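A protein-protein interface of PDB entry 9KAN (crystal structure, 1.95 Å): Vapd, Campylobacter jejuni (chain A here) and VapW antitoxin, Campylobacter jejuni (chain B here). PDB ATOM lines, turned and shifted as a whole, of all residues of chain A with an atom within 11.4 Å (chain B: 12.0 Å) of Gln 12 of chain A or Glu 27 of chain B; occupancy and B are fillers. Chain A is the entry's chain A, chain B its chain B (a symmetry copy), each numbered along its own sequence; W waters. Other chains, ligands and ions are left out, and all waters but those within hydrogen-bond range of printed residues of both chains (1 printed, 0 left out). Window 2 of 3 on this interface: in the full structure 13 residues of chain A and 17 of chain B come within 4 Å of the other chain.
Water W1 bridges OH of Tyr 31 of chain B (2.8 Å) and NH1 of Arg 18 of chain A (3.2 Å).
Hydrophobic or aromatic side chains of chain B within 4 Å of the printed part of chain A: Tyr 31 and Pro 32. Among the printed residues, 6 pairs touch across the chains.
The side-chain hydroxyl (OH) of Tyr 31 of chain B is in hydrogen-bond range of the side-chain carboxylate (OD1) of Asp 28 of chain B (3.3 Å). OG of Ser 63 of chain A sits at hydrogen-bond distance from O of Glu 65 of chain A, 2.6 Å away. The side-chain carboxylate (OD1) of Asp 25 of chain B lies close to the backbone NH (N) of Glu 27 of chain B, at 3.2 Å.
Of chain B, only Leu 26 (3.7 Å) and Glu 27 (3.0 Å) come within 4 Å of Gln 12 of chain A. Glu 27 of chain B touches just these residues of chain A: Gln 12, Glu 65 and Pro 66. No residue of chain B comes within 4 Å of Pro 14 of chain A. Of chain B, only Glu 27 comes within 4 Å of Pro 66 of chain A. No residue of chain A comes within 4 Å of Asp 25 of chain B. No residue of chain A comes within 4 Å of Leu 29 of chain B. Of the printed residues of chain A, Tyr 31 of chain B touches Glu 100. Of the printed residues of chain B, Glu 100 of chain A touches Tyr 31 and Pro 32. Of the printed residues of chain A, Pro 32 of chain B touches Glu 100 (3.2 Å). Lys 19 of chain A touches none of the printed residues of chain B. Lys 80 of chain B touches none of the printed residues of chain A. The nearest residue of chain A that does not touch Glu 27 of chain B is Asp 13 of chain A (5.1 Å).
Among the printed residues, merely in contact across the chains: Gln 12 of chain A with Glu 27 of chain B (3.0 Å), Glu 100 of chain A with Pro 32 of chain B (3.2 Å), Pro 66 of chain A with Glu 27 of chain B (3.5 Å), Glu 100 of chain A with Tyr 31 of chain B (3.5 Å), Glu 65 of chain A with Glu 27 of chain B (3.6 Å) and Gln 12 of chain A with Leu 26 of chain B (3.7 Å).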
ATOM      1  N   GLN A  12      14.283 -28.326 -23.938  1.00  0.00           N
ATOM      2  CA  GLN A  12      13.313 -28.061 -25.032  1.00  0.00           C
ATOM      3  C   GLN A  12      13.665 -26.730 -25.702  1.00  0.00           C
ATOM      4  O   GLN A  12      14.714 -26.668 -26.362  1.00  0.00           O
ATOM      5  CB  GLN A  12      11.890 -27.973 -24.486  1.00  0.00           C
ATOM      6  CG  GLN A  12      10.825 -28.520 -25.430  1.00  0.00           C
ATOM      7  CD  GLN A  12       9.869 -27.455 -25.920  1.00  0.00           C
ATOM      8  OE1 GLN A  12       9.843 -26.329 -25.413  1.00  0.00           O
ATOM      9  NE2 GLN A  12       9.071 -27.808 -26.918  1.00  0.00           N
ATOM     10  N   ASP A  13      12.809 -25.720 -25.544  1.00  0.00           N
ATOM     11  CA  ASP A  13      13.076 -24.370 -26.119  1.00  0.00           C
ATOM     12  C   ASP A  13      13.512 -23.444 -24.983  1.00  0.00           C
ATOM     13  O   ASP A  13      12.657 -23.035 -24.188  1.00  0.00           O
ATOM     14  CB  ASP A  13      11.899 -23.899 -26.953  1.00  0.00           C
ATOM     15  CG  ASP A  13      11.537 -24.787 -28.133  1.00  0.00           C
ATOM     16  OD1 ASP A  13      12.294 -25.741 -28.405  1.00  0.00           O
ATOM     17  OD2 ASP A  13      10.503 -24.514 -28.770  1.00  0.00           O
ATOM     18  N   PRO A  14      14.806 -23.086 -24.875  1.00  0.00           N
ATOM     19  CA  PRO A  14      15.296 -22.319 -23.713  1.00  0.00           C
ATOM     20  C   PRO A  14      14.701 -20.923 -23.598  1.00  0.00           C
ATOM     21  O   PRO A  14      14.638 -20.376 -22.492  1.00  0.00           O
ATOM     22  CB  PRO A  14      16.818 -22.286 -23.936  1.00  0.00           C
ATOM     23  CG  PRO A  14      17.006 -22.518 -25.382  1.00  0.00           C
ATOM     24  CD  PRO A  14      15.885 -23.409 -25.829  1.00  0.00           C
ATOM     25  N   GLY A  15      14.224 -20.347 -24.698  1.00  0.00           N
ATOM     26  CA  GLY A  15      13.552 -19.056 -24.616  1.00  0.00           C
ATOM     27  C   GLY A  15      12.238 -19.075 -23.845  1.00  0.00           C
ATOM     28  O   GLY A  15      11.764 -18.027 -23.397  1.00  0.00           O
ATOM     29  N   ILE A  16      11.631 -20.247 -23.675  1.00  0.00           N
ATOM     30  CA  ILE A  16      10.335 -20.336 -23.007  1.00  0.00           C
ATOM     31  C   ILE A  16      10.539 -20.650 -21.526  1.00  0.00           C
ATOM     32  O   ILE A  16      11.097 -21.697 -21.173  1.00  0.00           O
ATOM     33  CB  ILE A  16       9.456 -21.398 -23.687  1.00  0.00           C
ATOM     34  CG1 ILE A  16       9.170 -21.038 -25.152  1.00  0.00           C
ATOM     35  CG2 ILE A  16       8.163 -21.596 -22.920  1.00  0.00           C
ATOM     36  CD1 ILE A  16       8.304 -22.094 -25.868  1.00  0.00           C
ATOM     37  N   ASN A  17      10.055 -19.764 -20.653  1.00  0.00           N
ATOM     38  CA  ASN A  17      10.200 -19.898 -19.205  1.00  0.00           C
ATOM     39  C   ASN A  17       8.933 -20.435 -18.558  1.00  0.00           C
ATOM     40  O   ASN A  17       7.843 -20.433 -19.140  1.00  0.00           O
ATOM     41  CB  ASN A  17      10.508 -18.553 -18.535  1.00  0.00           C
ATOM     42  CG  ASN A  17      11.745 -17.883 -19.073  1.00  0.00           C
ATOM     43  OD1 ASN A  17      11.739 -16.675 -19.316  1.00  0.00           O
ATOM     44  ND2 ASN A  17      12.814 -18.648 -19.258  1.00  0.00           N
ATOM     45  N   ARG A  18       9.090 -20.854 -17.305  1.00  0.00           N
ATOM     46  CA  ARG A  18       7.959 -21.058 -16.424  1.00  0.00           C
ATOM     47  C   ARG A  18       7.276 -19.725 -16.140  1.00  0.00           C
ATOM     48  O   ARG A  18       7.848 -18.652 -16.332  1.00  0.00           O
ATOM     49  CB  ARG A  18       8.409 -21.718 -15.125  1.00  0.00           C
ATOM     50  CG  ARG A  18       8.375 -23.223 -15.195  1.00  0.00           C
ATOM     51  CD  ARG A  18       9.341 -23.915 -14.234  1.00  0.00           C
ATOM     52  NE  ARG A  18       9.197 -23.522 -12.837  1.00  0.00           N
ATOM     53  CZ  ARG A  18      10.206 -23.124 -12.066  1.00  0.00           C
ATOM     54  NH1 ARG A  18      11.450 -23.077 -12.520  1.00  0.00           N
ATOM     55  NH2 ARG A  18       9.961 -22.761 -10.806  1.00  0.00           N
ATOM     56  N   LYS A  19       6.017 -19.800 -15.702  1.00  0.00           N
ATOM     57  CA  LYS A  19       5.249 -18.595 -15.435  1.00  0.00           C
ATOM     58  C   LYS A  19       4.695 -18.625 -14.021  1.00  0.00           C
ATOM     59  O   LYS A  19       4.326 -19.685 -13.506  1.00  0.00           O
ATOM     60  CB  LYS A  19       4.112 -18.437 -16.436  1.00  0.00           C
ATOM     61  CG  LYS A  19       4.571 -18.461 -17.872  1.00  0.00           C
ATOM     62  CD  LYS A  19       5.031 -17.110 -18.355  1.00  0.00           C
ATOM     63  CE  LYS A  19       5.494 -17.195 -19.811  1.00  0.00           C
ATOM     64  NZ  LYS A  19       6.599 -18.154 -19.969  1.00  0.00           N
ATOM     65  N   SER A  63       3.680 -22.385 -13.013  1.00  0.00           N
ATOM     66  CA  SER A  63       3.520 -23.426 -14.019  1.00  0.00           C
ATOM     67  C   SER A  63       4.462 -24.590 -13.742  1.00  0.00           C
ATOM     68  O   SER A  63       5.645 -24.390 -13.443  1.00  0.00           O
ATOM     69  CB  SER A  63       3.781 -22.857 -15.410  1.00  0.00           C
ATOM     70  OG  SER A  63       5.150 -22.568 -15.586  1.00  0.00           O
ATOM     71  N   LYS A  64       3.936 -25.813 -13.852  1.00  0.00           N
ATOM     72  CA  LYS A  64       4.744 -26.998 -13.578  1.00  0.00           C
ATOM     73  C   LYS A  64       5.914 -27.097 -14.548  1.00  0.00           C
ATOM     74  O   LYS A  64       7.057 -27.337 -14.141  1.00  0.00           O
ATOM     75  CB  LYS A  64       3.866 -28.250 -13.634  1.00  0.00           C
ATOM     76  CG  LYS A  64       3.294 -28.674 -12.277  1.00  0.00           C
ATOM     77  CD  LYS A  64       1.901 -29.308 -12.373  1.00  0.00           C
ATOM     78  CE  LYS A  64       1.643 -29.941 -13.740  1.00  0.00           C
ATOM     79  NZ  LYS A  64       0.259 -30.492 -13.848  1.00  0.00           N
ATOM     80  N   GLU A  65       5.650 -26.885 -15.826  1.00  0.00           N
ATOM     81  CA  GLU A  65       6.634 -26.840 -16.890  1.00  0.00           C
ATOM     82  C   GLU A  65       6.737 -25.432 -17.446  1.00  0.00           C
ATOM     83  O   GLU A  65       5.911 -24.561 -17.129  1.00  0.00           O
ATOM     84  CB  GLU A  65       6.236 -27.815 -18.006  1.00  0.00           C
ATOM     85  CG  GLU A  65       5.904 -29.237 -17.542  1.00  0.00           C
ATOM     86  CD  GLU A  65       7.118 -30.007 -17.035  1.00  0.00           C
ATOM     87  OE1 GLU A  65       8.267 -29.610 -17.354  1.00  0.00           O
ATOM     88  OE2 GLU A  65       6.924 -31.015 -16.315  1.00  0.00           O
ATOM     89  N   PRO A  66       7.749 -25.147 -18.273  1.00  0.00           N
ATOM     90  CA  PRO A  66       7.744 -23.907 -19.053  1.00  0.00           C
ATOM     91  C   PRO A  66       6.511 -23.840 -19.940  1.00  0.00           C
ATOM     92  O   PRO A  66       6.052 -24.855 -20.460  1.00  0.00           O
ATOM     93  CB  PRO A  66       9.023 -24.008 -19.893  1.00  0.00           C
ATOM     94  CG  PRO A  66       9.940 -24.878 -19.078  1.00  0.00           C
ATOM     95  CD  PRO A  66       9.028 -25.884 -18.409  1.00  0.00           C
ATOM     96  N   ILE A  67       5.968 -22.633 -20.103  1.00  0.00           N
ATOM     97  CA  ILE A  67       4.766 -22.433 -20.915  1.00  0.00           C
ATOM     98  C   ILE A  67       4.881 -21.086 -21.620  1.00  0.00           C
ATOM     99  O   ILE A  67       5.231 -20.085 -20.989  1.00  0.00           O
ATOM    100  CB  ILE A  67       3.483 -22.535 -20.057  1.00  0.00           C
ATOM    101  CG1 ILE A  67       2.256 -22.077 -20.828  1.00  0.00           C
ATOM    102  CG2 ILE A  67       3.599 -21.730 -18.793  1.00  0.00           C
ATOM    103  CD1 ILE A  67       0.963 -22.584 -20.234  1.00  0.00           C
ATOM    104  N   ASN A  68       4.619 -21.056 -22.934  1.00  0.00           N
ATOM    105  CA  ASN A  68       4.811 -19.799 -23.640  1.00  0.00           C
ATOM    106  C   ASN A  68       3.656 -18.836 -23.348  1.00  0.00           C
ATOM    107  O   ASN A  68       2.619 -19.212 -22.789  1.00  0.00           O
ATOM    108  CB  ASN A  68       5.022 -20.013 -25.155  1.00  0.00           C
ATOM    109  CG  ASN A  68       3.802 -20.579 -25.880  1.00  0.00           C
ATOM    110  OD1 ASN A  68       2.662 -20.149 -25.675  1.00  0.00           O
ATOM    111  ND2 ASN A  68       4.048 -21.557 -26.745  1.00  0.00           N
ATOM    112  N   GLU A  69       3.874 -17.569 -23.715  1.00  0.00           N
ATOM    113  CA  GLU A  69       2.947 -16.502 -23.354  1.00  0.00           C
ATOM    114  C   GLU A  69       1.590 -16.677 -24.034  1.00  0.00           C
ATOM    115  O   GLU A  69       0.549 -16.339 -23.457  1.00  0.00           O
ATOM    116  CB  GLU A  69       3.546 -15.144 -23.732  1.00  0.00           C
ATOM    117  CG  GLU A  69       4.892 -14.828 -23.062  1.00  0.00           C
ATOM    118  CD  GLU A  69       4.771 -14.457 -21.600  1.00  0.00           C
ATOM    119  OE1 GLU A  69       3.654 -14.612 -21.041  1.00  0.00           O
ATOM    120  OE2 GLU A  69       5.795 -14.008 -21.012  1.00  0.00           O
ATOM    121  N   ARG A  71       0.012 -19.495 -24.771  1.00  0.00           N
ATOM    122  CA  ARG A  71      -0.778 -20.495 -24.057  1.00  0.00           C
ATOM    123  C   ARG A  71      -1.234 -19.996 -22.693  1.00  0.00           C
ATOM    124  O   ARG A  71      -2.335 -20.342 -22.243  1.00  0.00           O
ATOM    125  CB  ARG A  71       0.025 -21.788 -23.930  1.00  0.00           C
ATOM    126  CG  ARG A  71       0.186 -22.540 -25.275  1.00  0.00           C
ATOM    127  CD  ARG A  71       0.986 -23.834 -25.116  1.00  0.00           C
ATOM    128  NE  ARG A  71       2.397 -23.528 -24.910  1.00  0.00           N
ATOM    129  CZ  ARG A  71       3.227 -24.234 -24.149  1.00  0.00           C
ATOM    130  NH1 ARG A  71       2.826 -25.319 -23.500  1.00  0.00           N
ATOM    131  NH2 ARG A  71       4.492 -23.837 -24.033  1.00  0.00           N
ATOM    132  N   ILE A  98       9.438 -16.421 -15.017  1.00  0.00           N
ATOM    133  CA  ILE A  98      10.334 -16.970 -14.005  1.00  0.00           C
ATOM    134  C   ILE A  98      11.642 -17.342 -14.685  1.00  0.00           C
ATOM    135  O   ILE A  98      11.656 -18.151 -15.619  1.00  0.00           O
ATOM    136  CB  ILE A  98       9.709 -18.185 -13.298  1.00  0.00           C
ATOM    137  CG1 ILE A  98       8.474 -17.763 -12.517  1.00  0.00           C
ATOM    138  CG2 ILE A  98      10.719 -18.866 -12.386  1.00  0.00           C
ATOM    139  CD1 ILE A  98       8.577 -16.389 -11.911  1.00  0.00           C
ATOM    140  N   GLY A  99      12.740 -16.758 -14.212  1.00  0.00           N
ATOM    141  CA  GLY A  99      14.041 -16.913 -14.835  1.00  0.00           C
ATOM    142  C   GLY A  99      14.852 -18.055 -14.257  1.00  0.00           C
ATOM    143  O   GLY A  99      15.573 -18.749 -14.985  1.00  0.00           O
ATOM    144  N   GLU A 100      14.710 -18.257 -12.947  1.00  0.00           N
ATOM    145  CA  GLU A 100      15.357 -19.296 -12.155  1.00  0.00           C
ATOM    146  C   GLU A 100      14.769 -19.227 -10.753  1.00  0.00           C
ATOM    147  O   GLU A 100      14.452 -18.128 -10.293  1.00  0.00           O
ATOM    148  CB  GLU A 100      16.862 -19.074 -12.076  1.00  0.00           C
ATOM    149  CG  GLU A 100      17.619 -20.330 -12.121  1.00  0.00           C
ATOM    150  CD  GLU A 100      17.571 -20.914 -13.498  1.00  0.00           C
ATOM    151  OE1 GLU A 100      18.084 -20.239 -14.418  1.00  0.00           O
ATOM    152  OE2 GLU A 100      16.995 -22.019 -13.659  1.00  0.00           O
ATOM    153  N   ASP B  25      13.436 -35.493 -17.025  1.00  0.00           N
ATOM    154  CA  ASP B  25      13.032 -35.333 -18.423  1.00  0.00           C
ATOM    155  C   ASP B  25      13.900 -34.277 -19.093  1.00  0.00           C
ATOM    156  O   ASP B  25      15.028 -34.032 -18.667  1.00  0.00           O
ATOM    157  CB  ASP B  25      11.550 -34.953 -18.534  1.00  0.00           C
ATOM    158  CG  ASP B  25      11.259 -33.546 -18.023  1.00  0.00           C
ATOM    159  OD1 ASP B  25      12.007 -33.050 -17.148  1.00  0.00           O
ATOM    160  OD2 ASP B  25      10.278 -32.933 -18.494  1.00  0.00           O
ATOM    161  N   LEU B  26      13.364 -33.639 -20.131  1.00  0.00           N
ATOM    162  CA  LEU B  26      14.122 -32.678 -20.920  1.00  0.00           C
ATOM    163  C   LEU B  26      14.235 -31.297 -20.285  1.00  0.00           C
ATOM    164  O   LEU B  26      14.872 -30.428 -20.889  1.00  0.00           O
ATOM    165  CB  LEU B  26      13.495 -32.539 -22.308  1.00  0.00           C
ATOM    166  CG  LEU B  26      13.822 -33.658 -23.294  1.00  0.00           C
ATOM    167  CD1 LEU B  26      12.858 -33.628 -24.476  1.00  0.00           C
ATOM    168  CD2 LEU B  26      15.274 -33.526 -23.751  1.00  0.00           C
ATOM    169  N   GLU B  27      13.666 -31.065 -19.101  1.00  0.00           N
ATOM    170  CA  GLU B  27      13.595 -29.727 -18.523  1.00  0.00           C
ATOM    171  C   GLU B  27      14.372 -29.649 -17.205  1.00  0.00           C
ATOM    172  O   GLU B  27      14.702 -30.663 -16.585  1.00  0.00           O
ATOM    173  CB  GLU B  27      12.132 -29.300 -18.295  1.00  0.00           C
ATOM    174  CG  GLU B  27      11.205 -29.455 -19.504  1.00  0.00           C
ATOM    175  CD  GLU B  27      11.409 -28.376 -20.553  1.00  0.00           C
ATOM    176  OE1 GLU B  27      12.058 -27.353 -20.240  1.00  0.00           O
ATOM    177  OE2 GLU B  27      10.921 -28.555 -21.691  1.00  0.00           O
ATOM    178  N   ASP B  28      14.670 -28.407 -16.796  1.00  0.00           N
ATOM    179  CA  ASP B  28      15.226 -28.074 -15.473  1.00  0.00           C
ATOM    180  C   ASP B  28      16.690 -28.513 -15.308  1.00  0.00           C
ATOM    181  O   ASP B  28      17.173 -28.680 -14.182  1.00  0.00           O
ATOM    182  CB  ASP B  28      14.367 -28.670 -14.354  1.00  0.00           C
ATOM    183  CG  ASP B  28      14.405 -27.846 -13.084  1.00  0.00           C
ATOM    184  OD1 ASP B  28      15.006 -26.756 -13.099  1.00  0.00           O
ATOM    185  OD2 ASP B  28      13.831 -28.293 -12.065  1.00  0.00           O
ATOM    186  N   LEU B  29      17.428 -28.678 -16.410  1.00  0.00           N
ATOM    187  CA  LEU B  29      18.739 -29.311 -16.380  1.00  0.00           C
ATOM    188  C   LEU B  29      19.902 -28.347 -16.562  1.00  0.00           C
ATOM    189  O   LEU B  29      21.062 -28.777 -16.457  1.00  0.00           O
ATOM    190  CB  LEU B  29      18.813 -30.397 -17.459  1.00  0.00           C
ATOM    191  CG  LEU B  29      17.838 -31.563 -17.275  1.00  0.00           C
ATOM    192  CD1 LEU B  29      17.986 -32.569 -18.405  1.00  0.00           C
ATOM    193  CD2 LEU B  29      18.067 -32.234 -15.945  1.00  0.00           C
ATOM    194  N   ALA B  30      19.643 -27.055 -16.839  1.00  0.00           N
ATOM    195  CA  ALA B  30      20.704 -26.134 -17.266  1.00  0.00           C
ATOM    196  C   ALA B  30      20.615 -24.814 -16.494  1.00  0.00           C
ATOM    197  O   ALA B  30      20.111 -23.808 -16.995  1.00  0.00           O
ATOM    198  CB  ALA B  30      20.642 -25.921 -18.775  1.00  0.00           C
ATOM    199  N   TYR B  31      21.153 -24.807 -15.287  1.00  0.00           N
ATOM    200  CA  TYR B  31      21.239 -23.576 -14.512  1.00  0.00           C
ATOM    201  C   TYR B  31      22.453 -22.766 -14.956  1.00  0.00           C
ATOM    202  O   TYR B  31      23.455 -23.330 -15.409  1.00  0.00           O
ATOM    203  CB  TYR B  31      21.325 -23.903 -13.025  1.00  0.00           C
ATOM    204  CG  TYR B  31      19.987 -24.207 -12.380  1.00  0.00           C
ATOM    205  CD1 TYR B  31      19.245 -25.329 -12.753  1.00  0.00           C
ATOM    206  CD2 TYR B  31      19.461 -23.378 -11.392  1.00  0.00           C
ATOM    207  CE1 TYR B  31      18.027 -25.613 -12.171  1.00  0.00           C
ATOM    208  CE2 TYR B  31      18.239 -23.657 -10.792  1.00  0.00           C
ATOM    209  CZ  TYR B  31      17.530 -24.780 -11.183  1.00  0.00           C
ATOM    210  OH  TYR B  31      16.314 -25.078 -10.601  1.00  0.00           O
ATOM    211  N   PRO B  32      22.400 -21.438 -14.851  1.00  0.00           N
ATOM    212  CA  PRO B  32      23.584 -20.646 -15.204  1.00  0.00           C
ATOM    213  C   PRO B  32      24.697 -20.852 -14.183  1.00  0.00           C
ATOM    214  O   PRO B  32      24.448 -21.154 -13.013  1.00  0.00           O
ATOM    215  CB  PRO B  32      23.069 -19.200 -15.200  1.00  0.00           C
ATOM    216  CG  PRO B  32      21.880 -19.210 -14.366  1.00  0.00           C
ATOM    217  CD  PRO B  32      21.286 -20.603 -14.371  1.00  0.00           C
ATOM    218  N   LYS B  80      26.881 -26.973  -8.463  1.00  0.00           N
ATOM    219  CA  LYS B  80      26.382 -28.125  -9.210  1.00  0.00           C
ATOM    220  C   LYS B  80      25.388 -27.742 -10.305  1.00  0.00           C
ATOM    221  O   LYS B  80      25.197 -28.523 -11.248  1.00  0.00           O
ATOM    222  CB  LYS B  80      25.715 -29.128  -8.254  1.00  0.00           C
ATOM    223  CG  LYS B  80      26.638 -29.644  -7.151  1.00  0.00           C
ATOM    224  CD  LYS B  80      25.989 -30.733  -6.306  1.00  0.00           C
ATOM    225  CE  LYS B  80      27.043 -31.387  -5.423  1.00  0.00           C
ATOM    226  NZ  LYS B  80      26.500 -32.451  -4.560  1.00  0.00           N
ATOM    227  N   GLY B  81      24.747 -26.578 -10.204  1.00  0.00           N
ATOM    228  CA  GLY B  81      23.755 -26.194 -11.197  1.00  0.00           C
ATOM    229  C   GLY B  81      22.358 -26.744 -10.968  1.00  0.00           C
ATOM    230  O   GLY B  81      21.800 -27.435 -11.836  1.00  0.00           O
ATOM    231  N   ASP B  82      21.781 -26.433  -9.805  1.00  0.00           N
ATOM    232  CA  ASP B  82      20.413 -26.798  -9.456  1.00  0.00           C
ATOM    233  C   ASP B  82      19.874 -25.722  -8.517  1.00  0.00           C
ATOM    234  O   ASP B  82      20.502 -24.671  -8.317  1.00  0.00           O
ATOM    235  CB  ASP B  82      20.330 -28.201  -8.829  1.00  0.00           C
ATOM    236  CG  ASP B  82      21.101 -28.315  -7.496  1.00  0.00           C
ATOM    237  OD1 ASP B  82      21.168 -27.340  -6.717  1.00  0.00           O
ATOM    238  OD2 ASP B  82      21.667 -29.394  -7.229  1.00  0.00           O
ATOM    239  N   LYS B  83      18.722 -26.006  -7.904  1.00  0.00           N
ATOM    240  CA  LYS B  83      18.037 -24.956  -7.163  1.00  0.00           C
ATOM    241  C   LYS B  83      18.753 -24.557  -5.880  1.00  0.00           C
ATOM    242  O   LYS B  83      18.388 -23.530  -5.294  1.00  0.00           O
ATOM    243  CB  LYS B  83      16.599 -25.368  -6.852  1.00  0.00           C
ATOM    244  CG  LYS B  83      16.440 -26.490  -5.846  1.00  0.00           C
ATOM    245  CD  LYS B  83      14.985 -26.941  -5.808  1.00  0.00           C
ATOM    246  CE  LYS B  83      14.722 -27.948  -4.697  1.00  0.00           C
ATOM    247  NZ  LYS B  83      13.271 -28.346  -4.638  1.00  0.00           N
HETATM  248  O   HOH W   1      14.391 -23.165 -11.174  1.00  0.00           O
